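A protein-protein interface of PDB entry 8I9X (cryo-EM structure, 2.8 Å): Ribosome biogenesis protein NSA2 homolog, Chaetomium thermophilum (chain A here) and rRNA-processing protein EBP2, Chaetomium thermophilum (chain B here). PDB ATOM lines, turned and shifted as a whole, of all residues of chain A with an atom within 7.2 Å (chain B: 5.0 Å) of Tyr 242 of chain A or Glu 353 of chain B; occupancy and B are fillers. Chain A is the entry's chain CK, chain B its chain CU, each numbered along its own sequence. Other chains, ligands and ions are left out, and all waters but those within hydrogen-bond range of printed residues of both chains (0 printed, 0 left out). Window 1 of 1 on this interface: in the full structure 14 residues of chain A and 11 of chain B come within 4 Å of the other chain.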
ATOM      1  N   VAL A 184      12.475  16.636 -12.958  1.00  0.00           N
ATOM      2  CA  VAL A 184      13.916  16.820 -12.860  1.00  0.00           C
ATOM      3  C   VAL A 184      14.240  17.300 -11.456  1.00  0.00           C
ATOM      4  O   VAL A 184      13.623  18.249 -10.956  1.00  0.00           O
ATOM      5  CB  VAL A 184      14.425  17.813 -13.919  1.00  0.00           C
ATOM      6  CG1 VAL A 184      15.915  18.053 -13.750  1.00  0.00           C
ATOM      7  CG2 VAL A 184      14.113  17.301 -15.313  1.00  0.00           C
ATOM      8  N   LYS A 201      20.465  13.384 -25.771  1.00  0.00           N
ATOM      9  CA  LYS A 201      21.914  13.467 -26.056  1.00  0.00           C
ATOM     10  C   LYS A 201      22.554  12.080 -26.137  1.00  0.00           C
ATOM     11  O   LYS A 201      23.256  11.860 -27.131  1.00  0.00           O
ATOM     12  CB  LYS A 201      22.581  14.341 -24.994  1.00  0.00           C
ATOM     13  CG  LYS A 201      21.906  15.678 -24.729  1.00  0.00           C
ATOM     14  CD  LYS A 201      21.934  16.613 -25.913  1.00  0.00           C
ATOM     15  CE  LYS A 201      23.332  17.056 -26.282  1.00  0.00           C
ATOM     16  NZ  LYS A 201      23.318  18.027 -27.400  1.00  0.00           N
ATOM     17  N   ILE A 220      21.067  10.344 -20.815  1.00  0.00           N
ATOM     18  CA  ILE A 220      21.345  11.776 -20.779  1.00  0.00           C
ATOM     19  C   ILE A 220      20.397  12.500 -21.725  1.00  0.00           C
ATOM     20  O   ILE A 220      20.276  12.137 -22.900  1.00  0.00           O
ATOM     21  CB  ILE A 220      22.810  12.055 -21.145  1.00  0.00           C
ATOM     22  CG1 ILE A 220      23.743  11.437 -20.106  1.00  0.00           C
ATOM     23  CG2 ILE A 220      23.052  13.547 -21.261  1.00  0.00           C
ATOM     24  CD1 ILE A 220      23.627  12.062 -18.741  1.00  0.00           C
ATOM     25  N   ILE A 221      19.717  13.527 -21.212  1.00  0.00           N
ATOM     26  CA  ILE A 221      18.836  14.369 -22.005  1.00  0.00           C
ATOM     27  C   ILE A 221      19.137  15.826 -21.686  1.00  0.00           C
ATOM     28  O   ILE A 221      19.731  16.158 -20.658  1.00  0.00           O
ATOM     29  CB  ILE A 221      17.338  14.076 -21.767  1.00  0.00           C
ATOM     30  CG1 ILE A 221      16.930  14.462 -20.347  1.00  0.00           C
ATOM     31  CG2 ILE A 221      17.018  12.615 -22.039  1.00  0.00           C
ATOM     32  CD1 ILE A 221      15.439  14.467 -20.138  1.00  0.00           C
ATOM     33  N   GLU A 222      18.729  16.697 -22.602  1.00  0.00           N
ATOM     34  CA  GLU A 222      18.877  18.138 -22.457  1.00  0.00           C
ATOM     35  C   GLU A 222      17.572  18.697 -21.904  1.00  0.00           C
ATOM     36  O   GLU A 222      16.505  18.479 -22.488  1.00  0.00           O
ATOM     37  CB  GLU A 222      19.210  18.771 -23.808  1.00  0.00           C
ATOM     38  CG  GLU A 222      19.439  20.265 -23.783  1.00  0.00           C
ATOM     39  CD  GLU A 222      20.662  20.648 -22.981  1.00  0.00           C
ATOM     40  OE1 GLU A 222      21.583  19.813 -22.860  1.00  0.00           O
ATOM     41  OE2 GLU A 222      20.713  21.789 -22.485  1.00  0.00           O
ATOM     42  N   VAL A 223      17.649  19.411 -20.783  1.00  0.00           N
ATOM     43  CA  VAL A 223      16.460  19.914 -20.111  1.00  0.00           C
ATOM     44  C   VAL A 223      16.542  21.427 -19.983  1.00  0.00           C
ATOM     45  O   VAL A 223      17.609  22.000 -19.736  1.00  0.00           O
ATOM     46  CB  VAL A 223      16.253  19.261 -18.724  1.00  0.00           C
ATOM     47  CG1 VAL A 223      16.040  17.771 -18.870  1.00  0.00           C
ATOM     48  CG2 VAL A 223      17.441  19.537 -17.818  1.00  0.00           C
ATOM     49  N   VAL A 225      16.181  24.549 -17.999  1.00  0.00           N
ATOM     50  CA  VAL A 225      16.302  24.840 -16.575  1.00  0.00           C
ATOM     51  C   VAL A 225      16.073  26.325 -16.324  1.00  0.00           C
ATOM     52  O   VAL A 225      16.551  26.879 -15.328  1.00  0.00           O
ATOM     53  CB  VAL A 225      17.675  24.396 -16.043  1.00  0.00           C
ATOM     54  CG1 VAL A 225      17.825  22.892 -16.170  1.00  0.00           C
ATOM     55  CG2 VAL A 225      18.779  25.099 -16.806  1.00  0.00           C
ATOM     56  N   TRP A 239      19.783  28.192 -19.493  1.00  0.00           N
ATOM     57  CA  TRP A 239      18.632  27.829 -20.307  1.00  0.00           C
ATOM     58  C   TRP A 239      18.652  26.382 -20.769  1.00  0.00           C
ATOM     59  O   TRP A 239      17.726  25.960 -21.471  1.00  0.00           O
ATOM     60  CB  TRP A 239      18.535  28.771 -21.515  1.00  0.00           C
ATOM     61  CG  TRP A 239      18.113  30.145 -21.121  1.00  0.00           C
ATOM     62  CD1 TRP A 239      18.924  31.199 -20.821  1.00  0.00           C
ATOM     63  CD2 TRP A 239      16.773  30.642 -21.067  1.00  0.00           C
ATOM     64  NE1 TRP A 239      18.168  32.307 -20.525  1.00  0.00           N
ATOM     65  CE2 TRP A 239      16.843  31.993 -20.678  1.00  0.00           C
ATOM     66  CE3 TRP A 239      15.518  30.073 -21.298  1.00  0.00           C
ATOM     67  CZ2 TRP A 239      15.706  32.781 -20.508  1.00  0.00           C
ATOM     68  CZ3 TRP A 239      14.392  30.856 -21.129  1.00  0.00           C
ATOM     69  CH2 TRP A 239      14.494  32.195 -20.739  1.00  0.00           C
ATOM     70  N   GLY A 240      19.668  25.612 -20.398  1.00  0.00           N
ATOM     71  CA  GLY A 240      19.711  24.206 -20.738  1.00  0.00           C
ATOM     72  C   GLY A 240      20.828  23.468 -20.035  1.00  0.00           C
ATOM     73  O   GLY A 240      21.976  23.921 -20.039  1.00  0.00           O
ATOM     74  N   ARG A 241      20.507  22.327 -19.432  1.00  0.00           N
ATOM     75  CA  ARG A 241      21.497  21.518 -18.738  1.00  0.00           C
ATOM     76  C   ARG A 241      21.289  20.044 -19.049  1.00  0.00           C
ATOM     77  O   ARG A 241      20.297  19.643 -19.660  1.00  0.00           O
ATOM     78  CB  ARG A 241      21.456  21.728 -17.218  1.00  0.00           C
ATOM     79  CG  ARG A 241      21.777  23.136 -16.762  1.00  0.00           C
ATOM     80  CD  ARG A 241      23.189  23.522 -17.145  1.00  0.00           C
ATOM     81  NE  ARG A 241      23.553  24.834 -16.627  1.00  0.00           N
ATOM     82  CZ  ARG A 241      24.617  25.522 -17.015  1.00  0.00           C
ATOM     83  NH1 ARG A 241      25.430  25.065 -17.953  1.00  0.00           N
ATOM     84  NH2 ARG A 241      24.865  26.703 -16.457  1.00  0.00           N
ATOM     85  N   TYR A 242      22.261  19.241 -18.629  1.00  0.00           N
ATOM     86  CA  TYR A 242      22.178  17.799 -18.765  1.00  0.00           C
ATOM     87  C   TYR A 242      21.449  17.188 -17.576  1.00  0.00           C
ATOM     88  O   TYR A 242      21.687  17.549 -16.419  1.00  0.00           O
ATOM     89  CB  TYR A 242      23.575  17.193 -18.875  1.00  0.00           C
ATOM     90  CG  TYR A 242      24.246  17.421 -20.205  1.00  0.00           C
ATOM     91  CD1 TYR A 242      23.504  17.727 -21.333  1.00  0.00           C
ATOM     92  CD2 TYR A 242      25.624  17.346 -20.328  1.00  0.00           C
ATOM     93  CE1 TYR A 242      24.115  17.938 -22.550  1.00  0.00           C
ATOM     94  CE2 TYR A 242      26.243  17.559 -21.538  1.00  0.00           C
ATOM     95  CZ  TYR A 242      25.483  17.853 -22.646  1.00  0.00           C
ATOM     96  OH  TYR A 242      26.095  18.067 -23.859  1.00  0.00           O
ATOM     97  N   ALA A 243      20.570  16.237 -17.866  1.00  0.00           N
ATOM     98  CA  ALA A 243      19.877  15.501 -16.824  1.00  0.00           C
ATOM     99  C   ALA A 243      19.845  14.032 -17.202  1.00  0.00           C
ATOM    100  O   ALA A 243      19.566  13.686 -18.351  1.00  0.00           O
ATOM    101  CB  ALA A 243      18.453  16.026 -16.613  1.00  0.00           C
ATOM    102  N   GLN A 244      20.117  13.170 -16.233  1.00  0.00           N
ATOM    103  CA  GLN A 244      20.137  11.735 -16.466  1.00  0.00           C
ATOM    104  C   GLN A 244      18.802  11.141 -16.044  1.00  0.00           C
ATOM    105  O   GLN A 244      18.377  11.320 -14.897  1.00  0.00           O
ATOM    106  CB  GLN A 244      21.279  11.066 -15.706  1.00  0.00           C
ATOM    107  CG  GLN A 244      21.481   9.618 -16.098  1.00  0.00           C
ATOM    108  CD  GLN A 244      22.722   9.015 -15.489  1.00  0.00           C
ATOM    109  OE1 GLN A 244      23.456   8.280 -16.149  1.00  0.00           O
ATOM    110  NE2 GLN A 244      22.966   9.320 -14.222  1.00  0.00           N
ATOM    111  N   ALA A 257      14.367  12.415 -13.873  1.00  0.00           N
ATOM    112  CA  ALA A 257      15.739  12.772 -14.190  1.00  0.00           C
ATOM    113  C   ALA A 257      16.376  13.475 -13.004  1.00  0.00           C
ATOM    114  O   ALA A 257      15.713  14.164 -12.226  1.00  0.00           O
ATOM    115  CB  ALA A 257      15.814  13.670 -15.432  1.00  0.00           C
ATOM    116  N   VAL A 258      17.685  13.287 -12.876  1.00  0.00           N
ATOM    117  CA  VAL A 258      18.504  14.002 -11.906  1.00  0.00           C
ATOM    118  C   VAL A 258      19.436  14.919 -12.681  1.00  0.00           C
ATOM    119  O   VAL A 258      20.079  14.484 -13.643  1.00  0.00           O
ATOM    120  CB  VAL A 258      19.301  13.042 -11.005  1.00  0.00           C
ATOM    121  CG1 VAL A 258      20.273  13.814 -10.136  1.00  0.00           C
ATOM    122  CG2 VAL A 258      18.360  12.213 -10.150  1.00  0.00           C
ATOM    123  N   LEU A 259      19.499  16.184 -12.277  1.00  0.00           N
ATOM    124  CA  LEU A 259      20.242  17.179 -13.036  1.00  0.00           C
ATOM    125  C   LEU A 259      21.723  17.126 -12.673  1.00  0.00           C
ATOM    126  O   LEU A 259      22.088  17.132 -11.494  1.00  0.00           O
ATOM    127  CB  LEU A 259      19.665  18.565 -12.748  1.00  0.00           C
ATOM    128  CG  LEU A 259      20.130  19.778 -13.542  1.00  0.00           C
ATOM    129  CD1 LEU A 259      19.763  19.584 -14.990  1.00  0.00           C
ATOM    130  CD2 LEU A 259      19.502  21.045 -12.993  1.00  0.00           C
ATOM    131  N   LEU A 260      22.585  17.072 -13.692  1.00  0.00           N
ATOM    132  CA  LEU A 260      24.032  17.022 -13.474  1.00  0.00           C
ATOM    133  C   LEU A 260      24.573  18.449 -13.405  1.00  0.00           C
ATOM    134  O   LEU A 260      24.901  19.079 -14.411  1.00  0.00           O
ATOM    135  CB  LEU A 260      24.725  16.216 -14.566  1.00  0.00           C
ATOM    136  CG  LEU A 260      24.241  14.800 -14.882  1.00  0.00           C
ATOM    137  CD1 LEU A 260      23.377  14.777 -16.126  1.00  0.00           C
ATOM    138  CD2 LEU A 260      25.433  13.874 -15.046  1.00  0.00           C
ATOM    139  N   VAL A 261      24.671  18.956 -12.181  1.00  0.00           N
ATOM    140  CA  VAL A 261      25.179  20.302 -11.946  1.00  0.00           C
ATOM    141  C   VAL A 261      26.174  20.297 -10.794  1.00  0.00           C
ATOM    142  O   VAL A 261      26.104  19.450  -9.904  1.00  0.00           O
ATOM    143  CB  VAL A 261      24.032  21.291 -11.667  1.00  0.00           C
ATOM    144  CG1 VAL A 261      24.570  22.558 -11.019  1.00  0.00           C
ATOM    145  CG2 VAL A 261      23.294  21.622 -12.951  1.00  0.00           C
ATOM    146  N   LEU B 337      31.445  12.470 -15.267  1.00  0.00           N
ATOM    147  CA  LEU B 337      30.900  13.806 -15.483  1.00  0.00           C
ATOM    148  C   LEU B 337      30.119  14.283 -14.267  1.00  0.00           C
ATOM    149  O   LEU B 337      30.273  15.430 -13.831  1.00  0.00           O
ATOM    150  CB  LEU B 337      30.006  13.810 -16.723  1.00  0.00           C
ATOM    151  CG  LEU B 337      29.555  15.174 -17.243  1.00  0.00           C
ATOM    152  CD1 LEU B 337      30.741  15.942 -17.792  1.00  0.00           C
ATOM    153  CD2 LEU B 337      28.477  15.016 -18.302  1.00  0.00           C
ATOM    154  N   ARG B 341      31.076  17.499 -11.927  1.00  0.00           N
ATOM    155  CA  ARG B 341      30.136  18.593 -11.692  1.00  0.00           C
ATOM    156  C   ARG B 341      29.873  18.792 -10.207  1.00  0.00           C
ATOM    157  O   ARG B 341      29.774  19.935  -9.747  1.00  0.00           O
ATOM    158  CB  ARG B 341      28.818  18.343 -12.424  1.00  0.00           C
ATOM    159  CG  ARG B 341      28.923  18.237 -13.931  1.00  0.00           C
ATOM    160  CD  ARG B 341      29.284  19.571 -14.553  1.00  0.00           C
ATOM    161  NE  ARG B 341      29.399  19.479 -16.003  1.00  0.00           N
ATOM    162  CZ  ARG B 341      28.395  19.673 -16.845  1.00  0.00           C
ATOM    163  NH1 ARG B 341      27.178  19.962 -16.417  1.00  0.00           N
ATOM    164  NH2 ARG B 341      28.616  19.573 -18.153  1.00  0.00           N
ATOM    165  N   LEU B 349      30.216  26.980 -16.580  1.00  0.00           N
ATOM    166  CA  LEU B 349      29.609  26.755 -17.881  1.00  0.00           C
ATOM    167  C   LEU B 349      28.872  28.004 -18.358  1.00  0.00           C
ATOM    168  O   LEU B 349      28.806  29.024 -17.670  1.00  0.00           O
ATOM    169  CB  LEU B 349      28.656  25.564 -17.825  1.00  0.00           C
ATOM    170  CG  LEU B 349      29.303  24.181 -17.807  1.00  0.00           C
ATOM    171  CD1 LEU B 349      28.240  23.096 -17.776  1.00  0.00           C
ATOM    172  CD2 LEU B 349      30.218  24.004 -19.009  1.00  0.00           C
ATOM    173  N   ALA B 351      25.297  29.465 -20.819  1.00  0.00           N
ATOM    174  CA  ALA B 351      23.846  29.401 -20.711  1.00  0.00           C
ATOM    175  C   ALA B 351      23.312  28.031 -21.108  1.00  0.00           C
ATOM    176  O   ALA B 351      22.550  27.416 -20.359  1.00  0.00           O
ATOM    177  CB  ALA B 351      23.206  30.493 -21.572  1.00  0.00           C
ATOM    178  N   THR B 352      23.698  27.547 -22.281  1.00  0.00           N
ATOM    179  CA  THR B 352      23.308  26.235 -22.762  1.00  0.00           C
ATOM    180  C   THR B 352      24.491  25.276 -22.657  1.00  0.00           C
ATOM    181  O   THR B 352      25.549  25.611 -22.114  1.00  0.00           O
ATOM    182  CB  THR B 352      22.783  26.335 -24.194  1.00  0.00           C
ATOM    183  OG1 THR B 352      23.660  27.161 -24.970  1.00  0.00           O
ATOM    184  CG2 THR B 352      21.391  26.939 -24.206  1.00  0.00           C
ATOM    185  N   GLU B 353      24.316  24.066 -23.178  1.00  0.00           N
ATOM    186  CA  GLU B 353      25.376  23.063 -23.247  1.00  0.00           C
ATOM    187  C   GLU B 353      26.004  23.168 -24.631  1.00  0.00           C
ATOM    188  O   GLU B 353      25.410  23.747 -25.545  1.00  0.00           O
ATOM    189  CB  GLU B 353      24.833  21.662 -22.983  1.00  0.00           C
ATOM    190  CG  GLU B 353      24.219  21.472 -21.606  1.00  0.00           C
ATOM    191  CD  GLU B 353      25.261  21.261 -20.526  1.00  0.00           C
ATOM    192  OE1 GLU B 353      24.905  21.344 -19.332  1.00  0.00           O
ATOM    193  OE2 GLU B 353      26.434  21.010 -20.870  1.00  0.00           O
ATOM    194  N   ALA B 354      27.205  22.614 -24.784  1.00  0.00           N
ATOM    195  CA  ALA B 354      27.904  22.644 -26.061  1.00  0.00           C
ATOM    196  C   ALA B 354      27.110  21.908 -27.133  1.00  0.00           C
ATOM    197  O   ALA B 354      26.590  20.815 -26.889  1.00  0.00           O
ATOM    198  CB  ALA B 354      29.301  22.040 -25.915  1.00  0.00           C
ATOM    199  N   ASP B 355      27.009  22.499 -28.322  1.00  0.00           N
ATOM    200  CA  ASP B 355      26.204  21.950 -29.405  1.00  0.00           C
ATOM    201  C   ASP B 355      26.859  20.760 -30.095  1.00  0.00           C
ATOM    202  O   ASP B 355      26.197  20.083 -30.888  1.00  0.00           O
ATOM    203  CB  ASP B 355      25.899  23.040 -30.436  1.00  0.00           C
ATOM    204  CG  ASP B 355      24.955  24.099 -29.902  1.00  0.00           C
ATOM    205  OD1 ASP B 355      24.125  23.770 -29.028  1.00  0.00           O
ATOM    206  OD2 ASP B 355      25.042  25.260 -30.354  1.00  0.00           O
ATOM    207  N   PHE B 358      27.831  14.610 -27.841  1.00  0.00           N
ATOM    208  CA  PHE B 358      27.961  14.426 -26.374  1.00  0.00           C
ATOM    209  C   PHE B 358      29.288  13.775 -26.022  1.00  0.00           C
ATOM    210  O   PHE B 358      29.891  14.206 -25.036  1.00  0.00           O
ATOM    211  CB  PHE B 358      26.812  13.567 -25.852  1.00  0.00           C
ATOM    212  CG  PHE B 358      26.844  13.238 -24.382  1.00  0.00           C
ATOM    213  CD1 PHE B 358      26.430  14.160 -23.439  1.00  0.00           C
ATOM    214  CD2 PHE B 358      27.257  11.992 -23.947  1.00  0.00           C
ATOM    215  CE1 PHE B 358      26.454  13.850 -22.089  1.00  0.00           C
ATOM    216  CE2 PHE B 358      27.280  11.680 -22.598  1.00  0.00           C
ATOM    217  CZ  PHE B 358      26.872  12.609 -21.672  1.00  0.00           C
ATOM    218  N   ALA B 361      31.833  16.347 -26.394  1.00  0.00           N
ATOM    219  CA  ALA B 361      31.537  17.383 -25.390  1.00  0.00           C
ATOM    220  C   ALA B 361      32.023  16.891 -24.038  1.00  0.00           C
ATOM    221  O   ALA B 361      32.722  17.656 -23.358  1.00  0.00           O
ATOM    222  CB  ALA B 361      30.064  17.660 -25.355  1.00  0.00           C
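Of chain B, only Glu 353 (3.5 Å) and Phe 358 (3.8 Å) come within 4 Å of Tyr 242 of chain A.
Of chain A, only Glu 222 (3.4 Å), Gly 240 (3.7 Å), Arg 241 (3.5 Å) and Tyr 242 (3.5 Å) come within 4 Å of Glu 353 of chain B.
Printed residues of chain B within 4 Å of Trp 239 of chain A: Ala 351.
Of the printed residues of chain A, Leu 349 of chain B touches Arg 241.
Of the printed residues of chain A, Phe 358 of chain B touches Ile 220 (3.5 Å) and Tyr 242 (3.8 Å).
Val 223 of chain A touches none of the printed residues of chain B.
Asp 355 of chain B touches none of the printed residues of chain A.
The nearest residue of chain B that does not touch Tyr 242 of chain A is Ala 354 of chain B (4.1 Å).
The nearest printed residue of chain B that does not touch Arg 241 of chain A is Thr 352 of chain B (4.2 Å).
Printed residues of chain B that touch a printed residue of chain A: Arg 341, Leu 349, Ala 351, Thr 352, Glu 353 and Phe 358.
Hydrophobic or aromatic side chains of chain B within 4 Å of the printed part of chain A: Leu 349 and Phe 358.
Along chain B the printed residues that touch a printed residue of chain A span positions 341 to 358.
Hydrophobic or aromatic side chains of chain A that line the printed part of chain B: Ile 220 and Tyr 242.
Among the printed residues, 12 pairs touch across the chains.
Among the printed residues, no Asp or Glu carboxylate lies within 4 Å of a Lys or Arg side-chain nitrogen of the other chain.
N of Gly 240 of chain A lies within hydrogen-bond range of O of Ala 351 of chain B (3.4 Å).
NH1 of Arg 341 of chain B sits at hydrogen-bond distance from O of Leu 260 of chain A.
The backbone NH of Tyr 242 of chain A is in hydrogen-bond range of the side-chain carboxylate of Glu 353 of chain B (3.5 Å).
N of Trp 239 of chain A sits at hydrogen-bond distance from O of Ala 351 of chain B, 3.0 Å away.
The backbone NH of Lys 201 of chain A is in hydrogen-bond range of the backbone carbonyl oxygen of Ile 220 of chain A (3.1 Å).
The backbone NH (N) of Arg 241 of chain A lies within hydrogen-bond range of the side-chain carboxylate (OE2) of Glu 222 of chain A (3.1 Å).
O of Arg 241 of chain A is in hydrogen-bond range of N of Val 223 of chain A (2.9 Å).
The guanidinium group of Arg 341 of chain B lies within salt-bridge range of the side-chain carboxylate of Glu 353 of chain B (3.8 Å).
The backbone carbonyl oxygen (O) of Tyr 242 of chain A is in hydrogen-bond range of the backbone NH (N) of Leu 260 of chain A (2.9 Å).
Ile 220 of chain A touches Phe 358 of chain B.
CG of Glu 353 of chain B touches OE1 of Glu 222 of chain A, 3.4 Å away.
Gly 240 of chain A touches Thr 352 of chain B.
Gly 240 of chain A touches Glu 353 of chain B (O to CG, 3.7 Å).
Arg 241 of chain A touches Leu 349 of chain B.
Arg 241 of chain A touches Glu 353 of chain B (CA to OE1, 3.5 Å).
Phe 358 of chain B touches Tyr 242 of chain A (CE1 to CE2, 3.8 Å).
Arg 341 of chain B touches Val 261 of chain A.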
